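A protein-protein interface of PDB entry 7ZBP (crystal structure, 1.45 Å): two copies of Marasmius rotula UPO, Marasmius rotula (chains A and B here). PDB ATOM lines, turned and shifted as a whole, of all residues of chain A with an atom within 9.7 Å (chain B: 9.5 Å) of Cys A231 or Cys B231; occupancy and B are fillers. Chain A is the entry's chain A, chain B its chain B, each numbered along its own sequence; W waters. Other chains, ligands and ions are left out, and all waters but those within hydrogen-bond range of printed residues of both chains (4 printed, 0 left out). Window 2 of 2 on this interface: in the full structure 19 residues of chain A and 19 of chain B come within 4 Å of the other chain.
Among the printed residues, merely in contact across the chains: Gly A232 with Ala B233 (3.4 Å), Ala A233 with Gly B232 (3.7 Å), Ala A233 with Ala B233 (3.8 Å) and Cys A231 with Ala B233 (3.8 Å).
Hydrophobic or aromatic side chains of chain B that line the printed part of chain A: Ala B233.
Among the printed residues, 6 pairs touch across the chains.
Water W2 bridges O of Gly A232 (2.6 Å) and N of Ile B234 (3.0 Å).
Water W4 bridges O of Gly B232 (2.7 Å) and N of Ile A234 (3.0 Å).
Water W3 lies within hydrogen-bond range of the backbone NH of Gly A232 (2.8 Å) and the side-chain sulfur of Cys B231 (3.6 Å).
Water W1 lies within hydrogen-bond range of N of Gly B232 and SG of Cys A231.
Asp A152 touches none of the printed residues of chain B.
No residue of chain B comes within 4 Å of Asn A230.
Of chain B, only Cys B231 (2.1 Å), Gly B232 (3.4 Å) and Ala B233 (3.8 Å) come within 4 Å of Cys A231.
Gly A232 touches one residue of chain B.
Ala A233 touches just these residues of chain B: Gly B232 (3.7 Å) and Ala B233 (3.8 Å).
Trp B224 touches none of the printed residues of chain A.
No residue of chain A comes within 4 Å of Asn B230.
The backbone NH (N) of Cys A231 sits at hydrogen-bond distance from the side-chain carboxylate (OD1) of Asp A229.
The side-chain sulfur (SG) of Cys B231 lies close to the backbone NH (N) of Ala B233.
The side-chain sulfur of Cys A231 forms a disulfide with the side-chain sulfur of Cys B231.
SG of Cys A231 lies within hydrogen-bond range of N of Gly B232.
Cys A231 touches Gly B232, but with the chains exchanged Gly A232 does not touch Cys B231 (4.1 Å).
Cys A231 touches Ala B233, but with the chains exchanged Ala A233 does not touch Cys B231 (5.0 Å).
Gly A232 touches Ala B233, and with the chains exchanged Ala A233 touches Gly B232.
Ala B233 touches its own counterpart, Ala A233.
Positions printed for both chains: 86, 149, 150, 151, 152, 153, 154, 155, 224, 226, 227, 228, 229, 230, 231, 232, 233, 234 and 235.
Of the 6 pairs that touch across the chains among the printed residues, 4 have their exchanged pair printed and touching as well.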
ATOM      1  N   GLY A  86     -13.807 -19.125 -12.765  1.00  0.00           N
ATOM      2  CA  GLY A  86     -14.915 -19.386 -11.863  1.00  0.00           C
ATOM      3  C   GLY A  86     -16.222 -19.663 -12.565  1.00  0.00           C
ATOM      4  O   GLY A  86     -17.204 -19.793 -11.866  1.00  0.00           O
ATOM      5  N   THR A 149      -9.417 -21.563  -4.982  1.00  0.00           N
ATOM      6  CA  THR A 149     -10.824 -21.953  -4.804  1.00  0.00           C
ATOM      7  C   THR A 149     -10.941 -23.446  -5.017  1.00  0.00           C
ATOM      8  O   THR A 149     -10.496 -23.959  -6.054  1.00  0.00           O
ATOM      9  CB  THR A 149     -11.744 -21.210  -5.773  1.00  0.00           C
ATOM     10  OG1 THR A 149     -11.622 -19.822  -5.535  1.00  0.00           O
ATOM     11  CG2 THR A 149     -13.182 -21.618  -5.609  1.00  0.00           C
ATOM     12  N   ASN A 150     -11.490 -24.135  -4.039  1.00  0.00           N
ATOM     13  CA  ASN A 150     -11.617 -25.593  -4.061  1.00  0.00           C
ATOM     14  C   ASN A 150     -12.961 -25.930  -3.468  1.00  0.00           C
ATOM     15  O   ASN A 150     -13.133 -25.798  -2.231  1.00  0.00           O
ATOM     16  CB  ASN A 150     -10.511 -26.270  -3.242  1.00  0.00           C
ATOM     17  CG  ASN A 150     -10.749 -27.753  -3.098  1.00  0.00           C
ATOM     18  OD1 ASN A 150     -11.005 -28.459  -4.078  1.00  0.00           O
ATOM     19  ND2 ASN A 150     -10.667 -28.257  -1.863  1.00  0.00           N
ATOM     20  N   THR A 151     -13.927 -26.290  -4.277  1.00  0.00           N
ATOM     21  CA  THR A 151     -15.294 -26.599  -3.865  1.00  0.00           C
ATOM     22  C   THR A 151     -15.714 -27.975  -4.373  1.00  0.00           C
ATOM     23  O   THR A 151     -15.096 -28.542  -5.276  1.00  0.00           O
ATOM     24  CB  THR A 151     -16.268 -25.537  -4.379  1.00  0.00           C
ATOM     25  OG1 THR A 151     -16.396 -25.669  -5.809  1.00  0.00           O
ATOM     26  CG2 THR A 151     -15.865 -24.111  -4.049  1.00  0.00           C
ATOM     27  N   ASP A 152     -16.834 -28.487  -3.881  1.00  0.00           N
ATOM     28  CA  ASP A 152     -17.370 -29.771  -4.386  1.00  0.00           C
ATOM     29  C   ASP A 152     -17.593 -29.640  -5.898  1.00  0.00           C
ATOM     30  O   ASP A 152     -17.269 -30.591  -6.638  1.00  0.00           O
ATOM     31  CB  ASP A 152     -18.672 -30.088  -3.647  1.00  0.00           C
ATOM     32  CG  ASP A 152     -18.990 -31.561  -3.724  1.00  0.00           C
ATOM     33  OD1 ASP A 152     -18.416 -32.335  -2.904  1.00  0.00           O
ATOM     34  OD2 ASP A 152     -19.770 -31.930  -4.632  1.00  0.00           O
ATOM     35  N   LEU A 153     -18.029 -28.481  -6.357  1.00  0.00           N
ATOM     36  CA  LEU A 153     -18.234 -28.212  -7.803  1.00  0.00           C
ATOM     37  C   LEU A 153     -16.892 -28.257  -8.559  1.00  0.00           C
ATOM     38  O   LEU A 153     -16.827 -28.997  -9.581  1.00  0.00           O
ATOM     39  CB  LEU A 153     -18.936 -26.888  -8.056  1.00  0.00           C
ATOM     40  CG  LEU A 153     -19.140 -26.571  -9.531  1.00  0.00           C
ATOM     41  CD1 LEU A 153     -19.965 -27.633 -10.220  1.00  0.00           C
ATOM     42  CD2 LEU A 153     -19.783 -25.223  -9.710  1.00  0.00           C
ATOM     43  N   THR A 154     -15.879 -27.508  -8.139  1.00  0.00           N
ATOM     44  CA  THR A 154     -14.581 -27.560  -8.867  1.00  0.00           C
ATOM     45  C   THR A 154     -14.041 -28.974  -8.841  1.00  0.00           C
ATOM     46  O   THR A 154     -13.448 -29.426  -9.827  1.00  0.00           O
ATOM     47  CB  THR A 154     -13.556 -26.537  -8.388  1.00  0.00           C
ATOM     48  OG1 THR A 154     -13.197 -26.776  -7.030  1.00  0.00           O
ATOM     49  CG2 THR A 154     -14.108 -25.136  -8.524  1.00  0.00           C
ATOM     50  N   ALA A 155     -14.163 -29.696  -7.743  1.00  0.00           N
ATOM     51  CA  ALA A 155     -13.641 -31.074  -7.660  1.00  0.00           C
ATOM     52  C   ALA A 155     -14.379 -31.991  -8.658  1.00  0.00           C
ATOM     53  O   ALA A 155     -13.726 -32.864  -9.294  1.00  0.00           O
ATOM     54  CB  ALA A 155     -13.790 -31.588  -6.258  1.00  0.00           C
ATOM     55  N   TRP A 224     -10.303 -36.424  -1.870  1.00  0.00           N
ATOM     56  CA  TRP A 224     -10.732 -35.020  -1.814  1.00  0.00           C
ATOM     57  C   TRP A 224     -11.493 -34.744  -0.519  1.00  0.00           C
ATOM     58  O   TRP A 224     -12.346 -35.550  -0.125  1.00  0.00           O
ATOM     59  CB  TRP A 224     -11.582 -34.693  -3.020  1.00  0.00           C
ATOM     60  CG  TRP A 224     -11.913 -33.240  -3.063  1.00  0.00           C
ATOM     61  CD1 TRP A 224     -11.154 -32.250  -3.583  1.00  0.00           C
ATOM     62  CD2 TRP A 224     -13.086 -32.610  -2.504  1.00  0.00           C
ATOM     63  NE1 TRP A 224     -11.761 -31.054  -3.376  1.00  0.00           N
ATOM     64  CE2 TRP A 224     -12.947 -31.236  -2.735  1.00  0.00           C
ATOM     65  CE3 TRP A 224     -14.210 -33.083  -1.807  1.00  0.00           C
ATOM     66  CZ2 TRP A 224     -13.901 -30.298  -2.327  1.00  0.00           C
ATOM     67  CZ3 TRP A 224     -15.155 -32.171  -1.411  1.00  0.00           C
ATOM     68  CH2 TRP A 224     -15.010 -30.802  -1.679  1.00  0.00           C
ATOM     69  N   PRO A 226     -13.418 -31.064   1.593  1.00  0.00           N
ATOM     70  CA  PRO A 226     -13.635 -29.630   1.637  1.00  0.00           C
ATOM     71  C   PRO A 226     -12.540 -28.953   2.438  1.00  0.00           C
ATOM     72  O   PRO A 226     -12.000 -29.581   3.382  1.00  0.00           O
ATOM     73  CB  PRO A 226     -14.964 -29.469   2.381  1.00  0.00           C
ATOM     74  CG  PRO A 226     -15.625 -30.794   2.307  1.00  0.00           C
ATOM     75  CD  PRO A 226     -14.530 -31.834   2.163  1.00  0.00           C
ATOM     76  N   THR A 227     -12.187 -27.753   2.031  1.00  0.00           N
ATOM     77  CA  THR A 227     -11.084 -26.953   2.600  1.00  0.00           C
ATOM     78  C   THR A 227     -11.553 -25.571   3.033  1.00  0.00           C
ATOM     79  O   THR A 227     -10.754 -24.833   3.629  1.00  0.00           O
ATOM     80  CB  THR A 227      -9.936 -26.881   1.600  1.00  0.00           C
ATOM     81  OG1 THR A 227     -10.457 -26.413   0.341  1.00  0.00           O
ATOM     82  CG2 THR A 227      -9.232 -28.223   1.464  1.00  0.00           C
ATOM     83  N   GLY A 228     -12.733 -25.141   2.655  1.00  0.00           N
ATOM     84  CA  GLY A 228     -13.069 -23.734   2.934  1.00  0.00           C
ATOM     85  C   GLY A 228     -14.451 -23.472   2.445  1.00  0.00           C
ATOM     86  O   GLY A 228     -15.302 -24.339   2.671  1.00  0.00           O
ATOM     87  N   ASP A 229     -14.611 -22.348   1.767  1.00  0.00           N
ATOM     88  CA  ASP A 229     -15.851 -22.032   1.028  1.00  0.00           C
ATOM     89  C   ASP A 229     -16.093 -23.249   0.126  1.00  0.00           C
ATOM     90  O   ASP A 229     -15.189 -23.554  -0.673  1.00  0.00           O
ATOM     91  CB  ASP A 229     -15.734 -20.719   0.248  1.00  0.00           C
ATOM     92  CG  ASP A 229     -17.095 -20.206  -0.210  1.00  0.00           C
ATOM     93  OD1 ASP A 229     -18.039 -21.009  -0.282  1.00  0.00           O
ATOM     94  OD2 ASP A 229     -17.210 -18.989  -0.431  1.00  0.00           O
ATOM     95  N   ASN A 230     -17.175 -23.969   0.375  1.00  0.00           N
ATOM     96  CA  ASN A 230     -17.576 -25.190  -0.363  1.00  0.00           C
ATOM     97  C   ASN A 230     -18.823 -24.902  -1.220  1.00  0.00           C
ATOM     98  O   ASN A 230     -19.423 -25.836  -1.759  1.00  0.00           O
ATOM     99  CB  ASN A 230     -17.909 -26.357   0.556  1.00  0.00           C
ATOM    100  CG  ASN A 230     -17.707 -27.681  -0.143  1.00  0.00           C
ATOM    101  OD1 ASN A 230     -16.771 -27.789  -0.938  1.00  0.00           O
ATOM    102  ND2 ASN A 230     -18.520 -28.684   0.159  1.00  0.00           N
ATOM    103  N   CYS A 231     -19.207 -23.649  -1.304  1.00  0.00           N
ATOM    104  CA  CYS A 231     -20.366 -23.186  -2.122  1.00  0.00           C
ATOM    105  C   CYS A 231     -20.061 -23.351  -3.616  1.00  0.00           C
ATOM    106  O   CYS A 231     -19.123 -22.736  -4.103  1.00  0.00           O
ATOM    107  CB  CYS A 231     -20.659 -21.731  -1.793  1.00  0.00           C
ATOM    108  SG  CYS A 231     -22.130 -21.107  -2.646  1.00  0.00           S
ATOM    109  N   GLY A 232     -20.891 -24.114  -4.304  1.00  0.00           N
ATOM    110  CA  GLY A 232     -20.750 -24.321  -5.766  1.00  0.00           C
ATOM    111  C   GLY A 232     -21.218 -23.128  -6.588  1.00  0.00           C
ATOM    112  O   GLY A 232     -21.848 -23.356  -7.628  1.00  0.00           O
ATOM    113  N   ALA A 233     -20.930 -21.889  -6.184  1.00  0.00           N
ATOM    114  CA  ALA A 233     -21.374 -20.693  -6.947  1.00  0.00           C
ATOM    115  C   ALA A 233     -20.500 -20.583  -8.178  1.00  0.00           C
ATOM    116  O   ALA A 233     -19.290 -20.697  -8.069  1.00  0.00           O
ATOM    117  CB  ALA A 233     -21.336 -19.419  -6.164  1.00  0.00           C
ATOM    118  N   ILE A 234     -21.109 -20.367  -9.329  1.00  0.00           N
ATOM    119  CA  ILE A 234     -20.349 -20.040 -10.562  1.00  0.00           C
ATOM    120  C   ILE A 234     -20.497 -18.564 -10.896  1.00  0.00           C
ATOM    121  O   ILE A 234     -21.507 -17.923 -10.577  1.00  0.00           O
ATOM    122  CB  ILE A 234     -20.740 -20.918 -11.757  1.00  0.00           C
ATOM    123  CG1 ILE A 234     -22.177 -20.693 -12.214  1.00  0.00           C
ATOM    124  CG2 ILE A 234     -20.460 -22.399 -11.503  1.00  0.00           C
ATOM    125  CD1 ILE A 234     -22.396 -21.037 -13.692  1.00  0.00           C
ATOM    126  N   VAL A 235     -19.529 -18.072 -11.631  1.00  0.00           N
ATOM    127  CA  VAL A 235     -19.564 -16.766 -12.300  1.00  0.00           C
ATOM    128  C   VAL A 235     -20.561 -16.890 -13.461  1.00  0.00           C
ATOM    129  O   VAL A 235     -20.335 -17.717 -14.360  1.00  0.00           O
ATOM    130  CB  VAL A 235     -18.154 -16.331 -12.703  1.00  0.00           C
ATOM    131  CG1 VAL A 235     -18.165 -15.081 -13.560  1.00  0.00           C
ATOM    132  CG2 VAL A 235     -17.268 -16.147 -11.455  1.00  0.00           C
ATOM    133  N   GLY B  86     -34.184 -23.489  -8.339  1.00  0.00           N
ATOM    134  CA  GLY B  86     -32.802 -23.195  -7.955  1.00  0.00           C
ATOM    135  C   GLY B  86     -31.906 -22.852  -9.107  1.00  0.00           C
ATOM    136  O   GLY B  86     -30.700 -22.631  -8.854  1.00  0.00           O
ATOM    137  N   THR B 149     -35.084 -21.536   0.688  1.00  0.00           N
ATOM    138  CA  THR B 149     -33.772 -21.066   0.262  1.00  0.00           C
ATOM    139  C   THR B 149     -33.923 -19.571   0.057  1.00  0.00           C
ATOM    140  O   THR B 149     -34.852 -19.130  -0.651  1.00  0.00           O
ATOM    141  CB  THR B 149     -33.261 -21.747  -1.012  1.00  0.00           C
ATOM    142  OG1 THR B 149     -33.206 -23.158  -0.737  1.00  0.00           O
ATOM    143  CG2 THR B 149     -31.932 -21.172  -1.441  1.00  0.00           C
ATOM    144  N   ASN B 150     -33.083 -18.813   0.724  1.00  0.00           N
ATOM    145  CA  ASN B 150     -33.098 -17.343   0.748  1.00  0.00           C
ATOM    146  C   ASN B 150     -31.663 -16.872   0.877  1.00  0.00           C
ATOM    147  O   ASN B 150     -31.092 -16.938   2.007  1.00  0.00           O
ATOM    148  CB  ASN B 150     -33.967 -16.823   1.875  1.00  0.00           C
ATOM    149  CG  ASN B 150     -33.796 -15.359   2.169  1.00  0.00           C
ATOM    150  OD1 ASN B 150     -33.865 -14.541   1.283  1.00  0.00           O
ATOM    151  ND2 ASN B 150     -33.600 -15.018   3.443  1.00  0.00           N
ATOM    152  N   THR B 151     -31.127 -16.341  -0.205  1.00  0.00           N
ATOM    153  CA  THR B 151     -29.696 -15.996  -0.321  1.00  0.00           C
ATOM    154  C   THR B 151     -29.541 -14.669  -1.001  1.00  0.00           C
ATOM    155  O   THR B 151     -30.535 -14.110  -1.493  1.00  0.00           O
ATOM    156  CB  THR B 151     -28.970 -17.068  -1.113  1.00  0.00           C
ATOM    157  OG1 THR B 151     -29.401 -16.912  -2.471  1.00  0.00           O
ATOM    158  CG2 THR B 151     -29.277 -18.439  -0.581  1.00  0.00           C
ATOM    159  N   ASP B 152     -28.327 -14.132  -0.980  1.00  0.00           N
ATOM    160  CA  ASP B 152     -28.029 -12.878  -1.706  1.00  0.00           C
ATOM    161  C   ASP B 152     -28.560 -13.025  -3.137  1.00  0.00           C
ATOM    162  O   ASP B 152     -29.096 -12.061  -3.678  1.00  0.00           O
ATOM    163  CB  ASP B 152     -26.519 -12.632  -1.798  1.00  0.00           C
ATOM    164  CG  ASP B 152     -25.820 -12.188  -0.523  1.00  0.00           C
ATOM    165  OD1 ASP B 152     -26.510 -11.867   0.477  1.00  0.00           O
ATOM    166  OD2 ASP B 152     -24.583 -12.144  -0.559  1.00  0.00           O
ATOM    167  N   LEU B 153     -28.324 -14.174  -3.734  1.00  0.00           N
ATOM    168  CA  LEU B 153     -28.657 -14.357  -5.163  1.00  0.00           C
ATOM    169  C   LEU B 153     -30.187 -14.430  -5.318  1.00  0.00           C
ATOM    170  O   LEU B 153     -30.735 -13.691  -6.176  1.00  0.00           O
ATOM    171  CB  LEU B 153     -28.014 -15.628  -5.725  1.00  0.00           C
ATOM    172  CG  LEU B 153     -28.452 -15.934  -7.167  1.00  0.00           C
ATOM    173  CD1 LEU B 153     -28.082 -14.791  -8.103  1.00  0.00           C
ATOM    174  CD2 LEU B 153     -27.840 -17.224  -7.659  1.00  0.00           C
ATOM    175  N   THR B 154     -30.916 -15.178  -4.492  1.00  0.00           N
ATOM    176  CA  THR B 154     -32.401 -15.194  -4.662  1.00  0.00           C
ATOM    177  C   THR B 154     -32.978 -13.820  -4.338  1.00  0.00           C
ATOM    178  O   THR B 154     -33.951 -13.378  -4.990  1.00  0.00           O
ATOM    179  CB  THR B 154     -33.106 -16.277  -3.843  1.00  0.00           C
ATOM    180  OG1 THR B 154     -32.920 -16.062  -2.442  1.00  0.00           O
ATOM    181  CG2 THR B 154     -32.632 -17.675  -4.139  1.00  0.00           C
ATOM    182  N   ALA B 155     -32.453 -13.127  -3.324  1.00  0.00           N
ATOM    183  CA  ALA B 155     -32.956 -11.784  -2.985  1.00  0.00           C
ATOM    184  C   ALA B 155     -32.748 -10.809  -4.150  1.00  0.00           C
ATOM    185  O   ALA B 155     -33.650  -9.990  -4.445  1.00  0.00           O
ATOM    186  CB  ALA B 155     -32.316 -11.279  -1.722  1.00  0.00           C
ATOM    187  N   TRP B 224     -34.187  -6.939   4.688  1.00  0.00           N
ATOM    188  CA  TRP B 224     -33.781  -8.282   4.259  1.00  0.00           C
ATOM    189  C   TRP B 224     -32.585  -8.798   5.063  1.00  0.00           C
ATOM    190  O   TRP B 224     -31.611  -8.022   5.319  1.00  0.00           O
ATOM    191  CB  TRP B 224     -33.495  -8.304   2.761  1.00  0.00           C
ATOM    192  CG  TRP B 224     -33.122  -9.672   2.317  1.00  0.00           C
ATOM    193  CD1 TRP B 224     -33.966 -10.708   2.047  1.00  0.00           C
ATOM    194  CD2 TRP B 224     -31.792 -10.167   2.141  1.00  0.00           C
ATOM    195  NE1 TRP B 224     -33.236 -11.814   1.732  1.00  0.00           N
ATOM    196  CE2 TRP B 224     -31.906 -11.501   1.732  1.00  0.00           C
ATOM    197  CE3 TRP B 224     -30.532  -9.577   2.227  1.00  0.00           C
ATOM    198  CZ2 TRP B 224     -30.792 -12.282   1.466  1.00  0.00           C
ATOM    199  CZ3 TRP B 224     -29.434 -10.345   1.963  1.00  0.00           C
ATOM    200  CH2 TRP B 224     -29.567 -11.682   1.577  1.00  0.00           C
ATOM    201  N   PRO B 226     -30.192 -12.780   4.911  1.00  0.00           N
ATOM    202  CA  PRO B 226     -30.077 -14.144   4.404  1.00  0.00           C
ATOM    203  C   PRO B 226     -30.477 -15.224   5.426  1.00  0.00           C
ATOM    204  O   PRO B 226     -30.577 -14.936   6.604  1.00  0.00           O
ATOM    205  CB  PRO B 226     -28.595 -14.236   4.036  1.00  0.00           C
ATOM    206  CG  PRO B 226     -27.938 -13.329   5.031  1.00  0.00           C
ATOM    207  CD  PRO B 226     -28.874 -12.140   5.070  1.00  0.00           C
ATOM    208  N   THR B 227     -30.714 -16.430   4.917  1.00  0.00           N
ATOM    209  CA  THR B 227     -31.124 -17.683   5.618  1.00  0.00           C
ATOM    210  C   THR B 227     -30.053 -18.757   5.396  1.00  0.00           C
ATOM    211  O   THR B 227     -29.528 -18.891   4.273  1.00  0.00           O
ATOM    212  CB  THR B 227     -32.483 -18.188   5.105  1.00  0.00           C
ATOM    213  OG1 THR B 227     -33.469 -17.197   5.374  1.00  0.00           O
ATOM    214  CG2 THR B 227     -32.894 -19.506   5.721  1.00  0.00           C
ATOM    215  N   GLY B 228     -29.652 -19.458   6.464  1.00  0.00           N
ATOM    216  CA  GLY B 228     -28.778 -20.636   6.350  1.00  0.00           C
ATOM    217  C   GLY B 228     -27.413 -20.249   5.836  1.00  0.00           C
ATOM    218  O   GLY B 228     -26.942 -19.193   6.235  1.00  0.00           O
ATOM    219  N   ASP B 229     -26.831 -21.058   4.932  1.00  0.00           N
ATOM    220  CA  ASP B 229     -25.416 -20.927   4.485  1.00  0.00           C
ATOM    221  C   ASP B 229     -25.247 -19.814   3.454  1.00  0.00           C
ATOM    222  O   ASP B 229     -24.101 -19.516   3.087  1.00  0.00           O
ATOM    223  CB  ASP B 229     -24.896 -22.244   3.905  1.00  0.00           C
ATOM    224  CG  ASP B 229     -24.546 -23.235   5.010  1.00  0.00           C
ATOM    225  OD1 ASP B 229     -24.417 -22.788   6.188  1.00  0.00           O
ATOM    226  OD2 ASP B 229     -24.379 -24.429   4.700  1.00  0.00           O
ATOM    227  N   ASN B 230     -26.330 -19.212   2.993  1.00  0.00           N
ATOM    228  CA  ASN B 230     -26.232 -18.031   2.088  1.00  0.00           C
ATOM    229  C   ASN B 230     -25.335 -18.355   0.878  1.00  0.00           C
ATOM    230  O   ASN B 230     -24.453 -17.582   0.536  1.00  0.00           O
ATOM    231  CB  ASN B 230     -25.782 -16.743   2.784  1.00  0.00           C
ATOM    232  CG  ASN B 230     -25.992 -15.535   1.894  1.00  0.00           C
ATOM    233  OD1 ASN B 230     -26.756 -15.611   0.917  1.00  0.00           O
ATOM    234  ND2 ASN B 230     -25.367 -14.419   2.215  1.00  0.00           N
ATOM    235  N   CYS B 231     -25.568 -19.499   0.281  1.00  0.00           N
ATOM    236  CA  CYS B 231     -24.747 -20.008  -0.838  1.00  0.00           C
ATOM    237  C   CYS B 231     -25.420 -19.604  -2.146  1.00  0.00           C
ATOM    238  O   CYS B 231     -26.524 -20.064  -2.341  1.00  0.00           O
ATOM    239  CB  CYS B 231     -24.627 -21.516  -0.703  1.00  0.00           C
ATOM    240  SG  CYS B 231     -23.812 -22.284  -2.131  1.00  0.00           S
ATOM    241  N   GLY B 232     -24.719 -18.872  -3.008  1.00  0.00           N
ATOM    242  CA  GLY B 232     -25.208 -18.419  -4.340  1.00  0.00           C
ATOM    243  C   GLY B 232     -25.021 -19.434  -5.461  1.00  0.00           C
ATOM    244  O   GLY B 232     -24.958 -18.987  -6.616  1.00  0.00           O
ATOM    245  N   ALA B 233     -24.995 -20.724  -5.165  1.00  0.00           N
ATOM    246  CA  ALA B 233     -24.917 -21.840  -6.151  1.00  0.00           C
ATOM    247  C   ALA B 233     -26.269 -21.976  -6.866  1.00  0.00           C
ATOM    248  O   ALA B 233     -27.315 -21.877  -6.231  1.00  0.00           O
ATOM    249  CB  ALA B 233     -24.538 -23.116  -5.509  1.00  0.00           C
ATOM    250  N   ILE B 234     -26.234 -22.026  -8.193  1.00  0.00           N
ATOM    251  CA  ILE B 234     -27.428 -22.333  -9.007  1.00  0.00           C
ATOM    252  C   ILE B 234     -27.357 -23.780  -9.475  1.00  0.00           C
ATOM    253  O   ILE B 234     -26.274 -24.368  -9.629  1.00  0.00           O
ATOM    254  CB  ILE B 234     -27.621 -21.362 -10.177  1.00  0.00           C
ATOM    255  CG1 ILE B 234     -26.509 -21.454 -11.216  1.00  0.00           C
ATOM    256  CG2 ILE B 234     -27.823 -19.950  -9.691  1.00  0.00           C
ATOM    257  CD1 ILE B 234     -26.971 -20.976 -12.584  1.00  0.00           C
ATOM    258  N   VAL B 235     -28.507 -24.331  -9.767  1.00  0.00           N
ATOM    259  CA  VAL B 235     -28.703 -25.621 -10.441  1.00  0.00           C
ATOM    260  C   VAL B 235     -28.340 -25.419 -11.916  1.00  0.00           C
ATOM    261  O   VAL B 235     -28.896 -24.524 -12.562  1.00  0.00           O
ATOM    262  CB  VAL B 235     -30.139 -26.120 -10.237  1.00  0.00           C
ATOM    263  CG1 VAL B 235     -30.463 -27.334 -11.080  1.00  0.00           C
ATOM    264  CG2 VAL B 235     -30.369 -26.398  -8.748  1.00  0.00           C
HETATM  265  O   HOH W   1     -22.114 -17.650  -2.823  1.00  0.00           O
HETATM  266  O   HOH W   2     -23.603 -22.868  -9.431  1.00  0.00           O
HETATM  267  O   HOH W   3     -23.042 -25.576  -3.276  1.00  0.00           O
HETATM  268  O   HOH W   4     -23.952 -19.390  -9.139  1.00  0.00           O
